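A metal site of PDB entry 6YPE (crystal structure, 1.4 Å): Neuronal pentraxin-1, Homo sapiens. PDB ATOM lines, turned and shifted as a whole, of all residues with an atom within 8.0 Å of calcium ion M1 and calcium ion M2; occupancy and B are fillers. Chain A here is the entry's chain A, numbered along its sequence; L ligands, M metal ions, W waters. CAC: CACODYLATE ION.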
ATOM      1  N   THR A  45      24.016 -23.051  -5.822  1.00  0.00           N
ATOM      2  CA  THR A  45      23.269 -21.840  -6.152  1.00  0.00           C
ATOM      3  C   THR A  45      22.857 -21.065  -4.907  1.00  0.00           C
ATOM      4  O   THR A  45      21.798 -21.345  -4.321  1.00  0.00           O
ATOM      5  CB  THR A  45      22.032 -22.199  -6.971  1.00  0.00           C
ATOM      6  OG1 THR A  45      22.431 -22.933  -8.136  1.00  0.00           O
ATOM      7  CG2 THR A  45      21.295 -20.958  -7.431  1.00  0.00           C
ATOM      8  N   SER A  48      18.589 -17.580  -6.636  1.00  0.00           N
ATOM      9  CA  SER A  48      18.078 -17.436  -7.988  1.00  0.00           C
ATOM     10  C   SER A  48      16.780 -16.643  -7.958  1.00  0.00           C
ATOM     11  O   SER A  48      16.089 -16.576  -6.931  1.00  0.00           O
ATOM     12  CB  SER A  48      17.854 -18.794  -8.652  1.00  0.00           C
ATOM     13  OG  SER A  48      16.848 -19.536  -7.971  1.00  0.00           O
ATOM     14  N   TYR A  49      16.481 -16.034  -9.097  1.00  0.00           N
ATOM     15  CA  TYR A  49      15.324 -15.173  -9.269  1.00  0.00           C
ATOM     16  C   TYR A  49      14.702 -15.455 -10.623  1.00  0.00           C
ATOM     17  O   TYR A  49      15.384 -15.347 -11.649  1.00  0.00           O
ATOM     18  CB  TYR A  49      15.760 -13.705  -9.181  1.00  0.00           C
ATOM     19  CG  TYR A  49      14.663 -12.714  -9.461  1.00  0.00           C
ATOM     20  CD1 TYR A  49      13.617 -12.523  -8.549  1.00  0.00           C
ATOM     21  CD2 TYR A  49      14.684 -11.930 -10.608  1.00  0.00           C
ATOM     22  CE1 TYR A  49      12.628 -11.603  -8.795  1.00  0.00           C
ATOM     23  CE2 TYR A  49      13.690 -11.001 -10.864  1.00  0.00           C
ATOM     24  CZ  TYR A  49      12.661 -10.837  -9.946  1.00  0.00           C
ATOM     25  OH  TYR A  49      11.684  -9.919 -10.201  1.00  0.00           O
ATOM     26  N   ALA A  50      13.438 -15.882 -10.609  1.00  0.00           N
ATOM     27  CA  ALA A  50      12.680 -16.262 -11.783  1.00  0.00           C
ATOM     28  C   ALA A  50      11.501 -15.325 -11.997  1.00  0.00           C
ATOM     29  O   ALA A  50      10.836 -14.933 -11.043  1.00  0.00           O
ATOM     30  CB  ALA A  50      12.120 -17.670 -11.570  1.00  0.00           C
ATOM     31  N   GLN A  54      11.070 -16.399 -17.868  1.00  0.00           N
ATOM     32  CA  GLN A  54      12.524 -16.514 -17.726  1.00  0.00           C
ATOM     33  C   GLN A  54      12.844 -16.927 -16.291  1.00  0.00           C
ATOM     34  O   GLN A  54      12.937 -16.074 -15.398  1.00  0.00           O
ATOM     35  CB  GLN A  54      13.221 -15.214 -18.100  1.00  0.00           C
ATOM     36  CG  GLN A  54      14.730 -15.279 -17.944  1.00  0.00           C
ATOM     37  CD  GLN A  54      15.350 -16.419 -18.723  1.00  0.00           C
ATOM     38  OE1 GLN A  54      15.613 -17.491 -18.170  1.00  0.00           O
ATOM     39  NE2 GLN A  54      15.614 -16.198 -20.008  1.00  0.00           N
ATOM     40  N   ALA A  55      13.039 -18.218 -16.079  1.00  0.00           N
ATOM     41  CA  ALA A  55      13.378 -18.697 -14.754  1.00  0.00           C
ATOM     42  C   ALA A  55      14.799 -18.362 -14.339  1.00  0.00           C
ATOM     43  O   ALA A  55      15.119 -18.479 -13.151  1.00  0.00           O
ATOM     44  CB  ALA A  55      13.186 -20.202 -14.668  1.00  0.00           C
ATOM     45  N   ASN A  56      15.658 -17.964 -15.288  1.00  0.00           N
ATOM     46  CA  ASN A  56      17.040 -17.601 -14.995  1.00  0.00           C
ATOM     47  C   ASN A  56      17.225 -16.091 -15.125  1.00  0.00           C
ATOM     48  O   ASN A  56      18.174 -15.629 -15.757  1.00  0.00           O
ATOM     49  CB  ASN A  56      18.010 -18.297 -15.943  1.00  0.00           C
ATOM     50  CG  ASN A  56      17.999 -19.809 -15.810  1.00  0.00           C
ATOM     51  OD1 ASN A  56      17.306 -20.380 -14.962  1.00  0.00           O
ATOM     52  ND2 ASN A  56      18.777 -20.470 -16.663  1.00  0.00           N
ATOM     53  N   GLU A  57      16.329 -15.309 -14.522  1.00  0.00           N
ATOM     54  CA  GLU A  57      16.394 -13.862 -14.689  1.00  0.00           C
ATOM     55  C   GLU A  57      17.587 -13.272 -13.933  1.00  0.00           C
ATOM     56  O   GLU A  57      18.263 -12.371 -14.452  1.00  0.00           O
ATOM     57  CB  GLU A  57      15.066 -13.214 -14.259  1.00  0.00           C
ATOM     58  CG  GLU A  57      14.997 -11.715 -14.375  1.00  0.00           C
ATOM     59  CD  GLU A  57      15.106 -11.200 -15.806  1.00  0.00           C
ATOM     60  OE1 GLU A  57      15.147 -12.009 -16.756  1.00  0.00           O
ATOM     61  OE2 GLU A  57      15.146  -9.964 -15.965  1.00  0.00           O
ATOM     62  N   VAL A  59      20.681 -15.122 -11.390  1.00  0.00           N
ATOM     63  CA  VAL A  59      21.148 -16.356 -10.768  1.00  0.00           C
ATOM     64  C   VAL A  59      22.632 -16.224 -10.429  1.00  0.00           C
ATOM     65  O   VAL A  59      23.410 -15.684 -11.221  1.00  0.00           O
ATOM     66  CB  VAL A  59      20.985 -17.570 -11.703  1.00  0.00           C
ATOM     67  CG1 VAL A  59      21.191 -18.878 -10.927  1.00  0.00           C
ATOM     68  CG2 VAL A  59      19.643 -17.563 -12.393  1.00  0.00           C
ATOM     69  N   ILE A  61      25.565 -19.008  -9.430  1.00  0.00           N
ATOM     70  CA  ILE A  61      25.663 -20.468  -9.480  1.00  0.00           C
ATOM     71  C   ILE A  61      27.078 -20.912  -9.792  1.00  0.00           C
ATOM     72  O   ILE A  61      27.717 -20.413 -10.728  1.00  0.00           O
ATOM     73  CB  ILE A  61      24.660 -21.084 -10.483  1.00  0.00           C
ATOM     74  CG1 ILE A  61      24.844 -22.593 -10.517  1.00  0.00           C
ATOM     75  CG2 ILE A  61      24.845 -20.521 -11.874  1.00  0.00           C
ATOM     76  CD1 ILE A  61      23.709 -23.334 -11.207  1.00  0.00           C
ATOM     77  N   TRP A  63      28.221 -24.612 -10.646  1.00  0.00           N
ATOM     78  CA  TRP A  63      27.562 -25.895 -10.867  1.00  0.00           C
ATOM     79  C   TRP A  63      28.590 -26.931 -11.279  1.00  0.00           C
ATOM     80  O   TRP A  63      29.099 -26.897 -12.405  1.00  0.00           O
ATOM     81  CB  TRP A  63      26.478 -25.752 -11.931  1.00  0.00           C
ATOM     82  CG  TRP A  63      25.638 -26.987 -12.204  1.00  0.00           C
ATOM     83  CD1 TRP A  63      25.456 -28.085 -11.406  1.00  0.00           C
ATOM     84  CD2 TRP A  63      24.859 -27.212 -13.377  1.00  0.00           C
ATOM     85  NE1 TRP A  63      24.601 -28.978 -12.012  1.00  0.00           N
ATOM     86  CE2 TRP A  63      24.211 -28.461 -13.213  1.00  0.00           C
ATOM     87  CE3 TRP A  63      24.613 -26.479 -14.540  1.00  0.00           C
ATOM     88  CZ2 TRP A  63      23.367 -28.991 -14.194  1.00  0.00           C
ATOM     89  CZ3 TRP A  63      23.776 -26.998 -15.503  1.00  0.00           C
ATOM     90  CH2 TRP A  63      23.152 -28.245 -15.321  1.00  0.00           C
ATOM     91  N   LEU A  71      24.177 -15.106 -13.848  1.00  0.00           N
ATOM     92  CA  LEU A  71      23.308 -15.097 -15.018  1.00  0.00           C
ATOM     93  C   LEU A  71      22.319 -13.951 -14.862  1.00  0.00           C
ATOM     94  O   LEU A  71      21.732 -13.791 -13.791  1.00  0.00           O
ATOM     95  CB  LEU A  71      22.493 -16.383 -15.183  1.00  0.00           C
ATOM     96  CG  LEU A  71      23.119 -17.736 -14.955  1.00  0.00           C
ATOM     97  CD1 LEU A  71      22.105 -18.837 -15.277  1.00  0.00           C
ATOM     98  CD2 LEU A  71      24.250 -17.847 -15.845  1.00  0.00           C
ATOM     99  N   ASP A  74      19.384 -15.152 -18.381  1.00  0.00           N
ATOM    100  CA  ASP A  74      19.994 -16.357 -18.921  1.00  0.00           C
ATOM    101  C   ASP A  74      21.250 -16.072 -19.751  1.00  0.00           C
ATOM    102  O   ASP A  74      21.600 -16.856 -20.638  1.00  0.00           O
ATOM    103  CB  ASP A  74      19.001 -17.214 -19.718  1.00  0.00           C
ATOM    104  CG  ASP A  74      19.480 -18.633 -19.902  1.00  0.00           C
ATOM    105  OD1 ASP A  74      20.097 -19.194 -18.957  1.00  0.00           O
ATOM    106  OD2 ASP A  74      19.241 -19.197 -20.986  1.00  0.00           O
ATOM    107  N   GLN A 133      18.640 -22.673  -4.046  1.00  0.00           N
ATOM    108  CA  GLN A 133      18.271 -23.525  -5.170  1.00  0.00           C
ATOM    109  C   GLN A 133      18.195 -22.693  -6.436  1.00  0.00           C
ATOM    110  O   GLN A 133      17.945 -21.481  -6.405  1.00  0.00           O
ATOM    111  CB  GLN A 133      16.900 -24.173  -4.974  1.00  0.00           C
ATOM    112  CG  GLN A 133      16.737 -25.069  -3.755  1.00  0.00           C
ATOM    113  CD  GLN A 133      17.399 -26.438  -3.902  1.00  0.00           C
ATOM    114  OE1 GLN A 133      17.717 -26.884  -5.008  1.00  0.00           O
ATOM    115  NE2 GLN A 133      17.602 -27.108  -2.781  1.00  0.00           N
ATOM    116  N   GLU A 134      18.375 -23.381  -7.565  1.00  0.00           N
ATOM    117  CA  GLU A 134      18.237 -22.843  -8.911  1.00  0.00           C
ATOM    118  C   GLU A 134      16.846 -23.192  -9.423  1.00  0.00           C
ATOM    119  O   GLU A 134      16.369 -24.315  -9.228  1.00  0.00           O
ATOM    120  CB  GLU A 134      19.290 -23.516  -9.804  1.00  0.00           C
ATOM    121  CG  GLU A 134      19.738 -22.730 -11.044  1.00  0.00           C
ATOM    122  CD  GLU A 134      18.772 -22.782 -12.210  1.00  0.00           C
ATOM    123  OE1 GLU A 134      18.657 -21.761 -12.921  1.00  0.00           O
ATOM    124  OE2 GLU A 134      18.145 -23.843 -12.444  1.00  0.00           O
ATOM    125  N   GLN A 135      16.182 -22.220 -10.060  1.00  0.00           N
ATOM    126  CA  GLN A 135      14.809 -22.385 -10.505  1.00  0.00           C
ATOM    127  C   GLN A 135      14.725 -22.735 -11.993  1.00  0.00           C
ATOM    128  O   GLN A 135      15.413 -22.134 -12.819  1.00  0.00           O
ATOM    129  CB  GLN A 135      13.996 -21.121 -10.241  1.00  0.00           C
ATOM    130  CG  GLN A 135      13.702 -20.890  -8.783  1.00  0.00           C
ATOM    131  CD  GLN A 135      13.090 -19.530  -8.514  1.00  0.00           C
ATOM    132  OE1 GLN A 135      11.877 -19.327  -8.633  1.00  0.00           O
ATOM    133  NE2 GLN A 135      13.937 -18.583  -8.155  1.00  0.00           N
ATOM    134  N   ASP A 136      13.878 -23.718 -12.311  1.00  0.00           N
ATOM    135  CA  ASP A 136      13.517 -24.016 -13.688  1.00  0.00           C
ATOM    136  C   ASP A 136      12.053 -23.712 -13.969  1.00  0.00           C
ATOM    137  O   ASP A 136      11.645 -23.736 -15.137  1.00  0.00           O
ATOM    138  CB  ASP A 136      13.857 -25.477 -14.039  1.00  0.00           C
ATOM    139  CG  ASP A 136      15.347 -25.748 -14.027  1.00  0.00           C
ATOM    140  OD1 ASP A 136      16.118 -24.775 -14.179  1.00  0.00           O
ATOM    141  OD2 ASP A 136      15.752 -26.912 -13.851  1.00  0.00           O
ATOM    142  N   THR A 137      11.274 -23.407 -12.925  1.00  0.00           N
ATOM    143  CA  THR A 137       9.920 -22.901 -13.061  1.00  0.00           C
ATOM    144  C   THR A 137       9.784 -21.732 -12.093  1.00  0.00           C
ATOM    145  O   THR A 137      10.657 -21.485 -11.263  1.00  0.00           O
ATOM    146  CB  THR A 137       8.885 -23.971 -12.709  1.00  0.00           C
ATOM    147  OG1 THR A 137       8.982 -24.288 -11.319  1.00  0.00           O
ATOM    148  CG2 THR A 137       9.123 -25.253 -13.495  1.00  0.00           C
ATOM    149  N   GLY A 140      10.123 -22.742  -8.445  1.00  0.00           N
ATOM    150  CA  GLY A 140      10.343 -24.165  -8.257  1.00  0.00           C
ATOM    151  C   GLY A 140      11.202 -24.799  -9.333  1.00  0.00           C
ATOM    152  O   GLY A 140      12.035 -24.144  -9.952  1.00  0.00           O
ATOM    153  N   GLY A 141      10.987 -26.088  -9.579  1.00  0.00           N
ATOM    154  CA  GLY A 141      11.790 -26.807 -10.538  1.00  0.00           C
ATOM    155  C   GLY A 141      13.244 -26.930 -10.108  1.00  0.00           C
ATOM    156  O   GLY A 141      14.147 -26.683 -10.906  1.00  0.00           O
ATOM    157  N   PHE A 142      13.473 -27.325  -8.858  1.00  0.00           N
ATOM    158  CA  PHE A 142      14.802 -27.395  -8.275  1.00  0.00           C
ATOM    159  C   PHE A 142      15.551 -28.674  -8.696  1.00  0.00           C
ATOM    160  O   PHE A 142      14.956 -29.723  -8.983  1.00  0.00           O
ATOM    161  CB  PHE A 142      14.715 -27.339  -6.752  1.00  0.00           C
ATOM    162  CG  PHE A 142      14.007 -26.142  -6.209  1.00  0.00           C
ATOM    163  CD1 PHE A 142      14.034 -24.909  -6.850  1.00  0.00           C
ATOM    164  CD2 PHE A 142      13.305 -26.219  -5.009  1.00  0.00           C
ATOM    165  CE1 PHE A 142      13.377 -23.801  -6.318  1.00  0.00           C
ATOM    166  CE2 PHE A 142      12.660 -25.129  -4.480  1.00  0.00           C
ATOM    167  CZ  PHE A 142      12.702 -23.911  -5.135  1.00  0.00           C
ATOM    168  N   ASP A 143      16.878 -28.580  -8.649  1.00  0.00           N
ATOM    169  CA  ASP A 143      17.795 -29.626  -9.085  1.00  0.00           C
ATOM    170  C   ASP A 143      18.852 -29.774  -8.008  1.00  0.00           C
ATOM    171  O   ASP A 143      19.639 -28.854  -7.765  1.00  0.00           O
ATOM    172  CB  ASP A 143      18.442 -29.206 -10.418  1.00  0.00           C
ATOM    173  CG  ASP A 143      19.464 -30.218 -10.934  1.00  0.00           C
ATOM    174  OD1 ASP A 143      19.912 -31.098 -10.186  1.00  0.00           O
ATOM    175  OD2 ASP A 143      19.844 -30.073 -12.117  1.00  0.00           O
ATOM    176  N   ALA A 144      18.869 -30.934  -7.336  1.00  0.00           N
ATOM    177  CA  ALA A 144      19.788 -31.132  -6.228  1.00  0.00           C
ATOM    178  C   ALA A 144      21.238 -30.936  -6.628  1.00  0.00           C
ATOM    179  O   ALA A 144      22.053 -30.516  -5.811  1.00  0.00           O
ATOM    180  CB  ALA A 144      19.597 -32.517  -5.603  1.00  0.00           C
ATOM    181  N   THR A 145      21.599 -31.242  -7.888  1.00  0.00           N
ATOM    182  CA  THR A 145      23.003 -31.080  -8.270  1.00  0.00           C
ATOM    183  C   THR A 145      23.414 -29.620  -8.325  1.00  0.00           C
ATOM    184  O   THR A 145      24.626 -29.334  -8.332  1.00  0.00           O
ATOM    185  CB  THR A 145      23.316 -31.752  -9.612  1.00  0.00           C
ATOM    186  OG1 THR A 145      22.760 -30.984 -10.691  1.00  0.00           O
ATOM    187  CG2 THR A 145      22.768 -33.170  -9.645  1.00  0.00           C
ATOM    188  N   GLN A 146      22.457 -28.696  -8.361  1.00  0.00           N
ATOM    189  CA  GLN A 146      22.688 -27.261  -8.386  1.00  0.00           C
ATOM    190  C   GLN A 146      22.465 -26.613  -7.029  1.00  0.00           C
ATOM    191  O   GLN A 146      22.690 -25.409  -6.894  1.00  0.00           O
ATOM    192  CB  GLN A 146      21.766 -26.608  -9.423  1.00  0.00           C
ATOM    193  CG  GLN A 146      22.060 -27.048 -10.855  1.00  0.00           C
ATOM    194  CD  GLN A 146      21.085 -26.499 -11.881  1.00  0.00           C
ATOM    195  OE1 GLN A 146      19.876 -26.447 -11.648  1.00  0.00           O
ATOM    196  NE2 GLN A 146      21.603 -26.128 -13.036  1.00  0.00           N
HETATM  197 AS   CAC L   1      19.769 -24.347 -15.883  1.00  0.00          AS
HETATM  198  O1  CAC L   1      19.353 -25.617 -14.763  1.00  0.00           O
HETATM  199  O2  CAC L   1      18.458 -23.222 -16.080  1.00  0.00           O
HETATM  200  C1  CAC L   1      21.257 -23.297 -15.128  1.00  0.00           C
HETATM  201  C2  CAC L   1      20.312 -25.119 -17.614  1.00  0.00           C
HETATM  202 CA    CA M   1      18.022 -26.062 -13.072  1.00  0.00          CA
HETATM  203 CA    CA M   2      17.014 -22.596 -14.390  1.00  0.00          CA
HETATM  204  O   HOH W   1      15.583 -22.459 -16.286  1.00  0.00           O
HETATM  205  O   HOH W   2      18.431 -28.352 -13.638  1.00  0.00           O
HETATM  206  O   HOH W   3      16.752 -26.262 -11.032  1.00  0.00           O
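Calcium ion M1 is bound by O1 of the ligand (2.2 Å).
OE2 of Glu 134 binds calcium ion M1.
The side-chain amide oxygen (OE1) of Gln 146 is bound to calcium ion M1 (2.4 Å).
Calcium ion M1 is bound by water W2 (2.4 Å).
Water W3 binds calcium ion M1 (2.4 Å).
Calcium ion M1 is bound by the side-chain carboxylate (OD2) of Asp 136 (2.5 Å).
Calcium ion M1 is bound by OD1 of Asp 136.
Three residues have an atom within 4 Å of calcium ion M1: Glu 134, Asp 136 and Gln 146.
Of the 25 residues printed, 4 come within 4 Å of calcium ion M2.
The nearest printed residue that does not touch calcium ion M2 is Ala 55 (4.5 Å).
Calcium ion M2 is bound by the backbone carbonyl oxygen (O) of Gln 135 (2.3 Å), the side-chain amide oxygen (OD1) of Asn 56 (2.3 Å), an oxygen (O2) of the ligand (2.3 Å), the side-chain carboxylate (OE1) of Glu 134 (2.4 Å), the side-chain carboxylate (OD1) of Asp 136 (2.4 Å), water W1 (2.4 Å) and the side-chain carboxylate (OE2) of Glu 134 (2.6 Å).
NE2 of Gln 135 lies within hydrogen-bond range of OG of Ser 48 (3.1 Å).
The backbone NH (N) of Asn 56 is in hydrogen-bond range of the side-chain amide oxygen (OE1) of Gln 54, at 2.9 Å.
The backbone carbonyl oxygen (O) of Gln 146 is in hydrogen-bond range of the side-chain hydroxyl (OG1) of Thr 45 (2.8 Å).
N of Asp 136 is in hydrogen-bond range of O of Gly 141 (3.3 Å).
The backbone carbonyl oxygen (O) of Asn 56 sits at hydrogen-bond distance from the backbone NH (N) of Asp 74.
Water W3 lies within hydrogen-bond range of the backbone carbonyl oxygen (O) of Gly 141 (2.6 Å), the backbone carbonyl oxygen (O) of Glu 134 (2.7 Å) and the backbone NH (N) of Asp 143 (3.3 Å).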
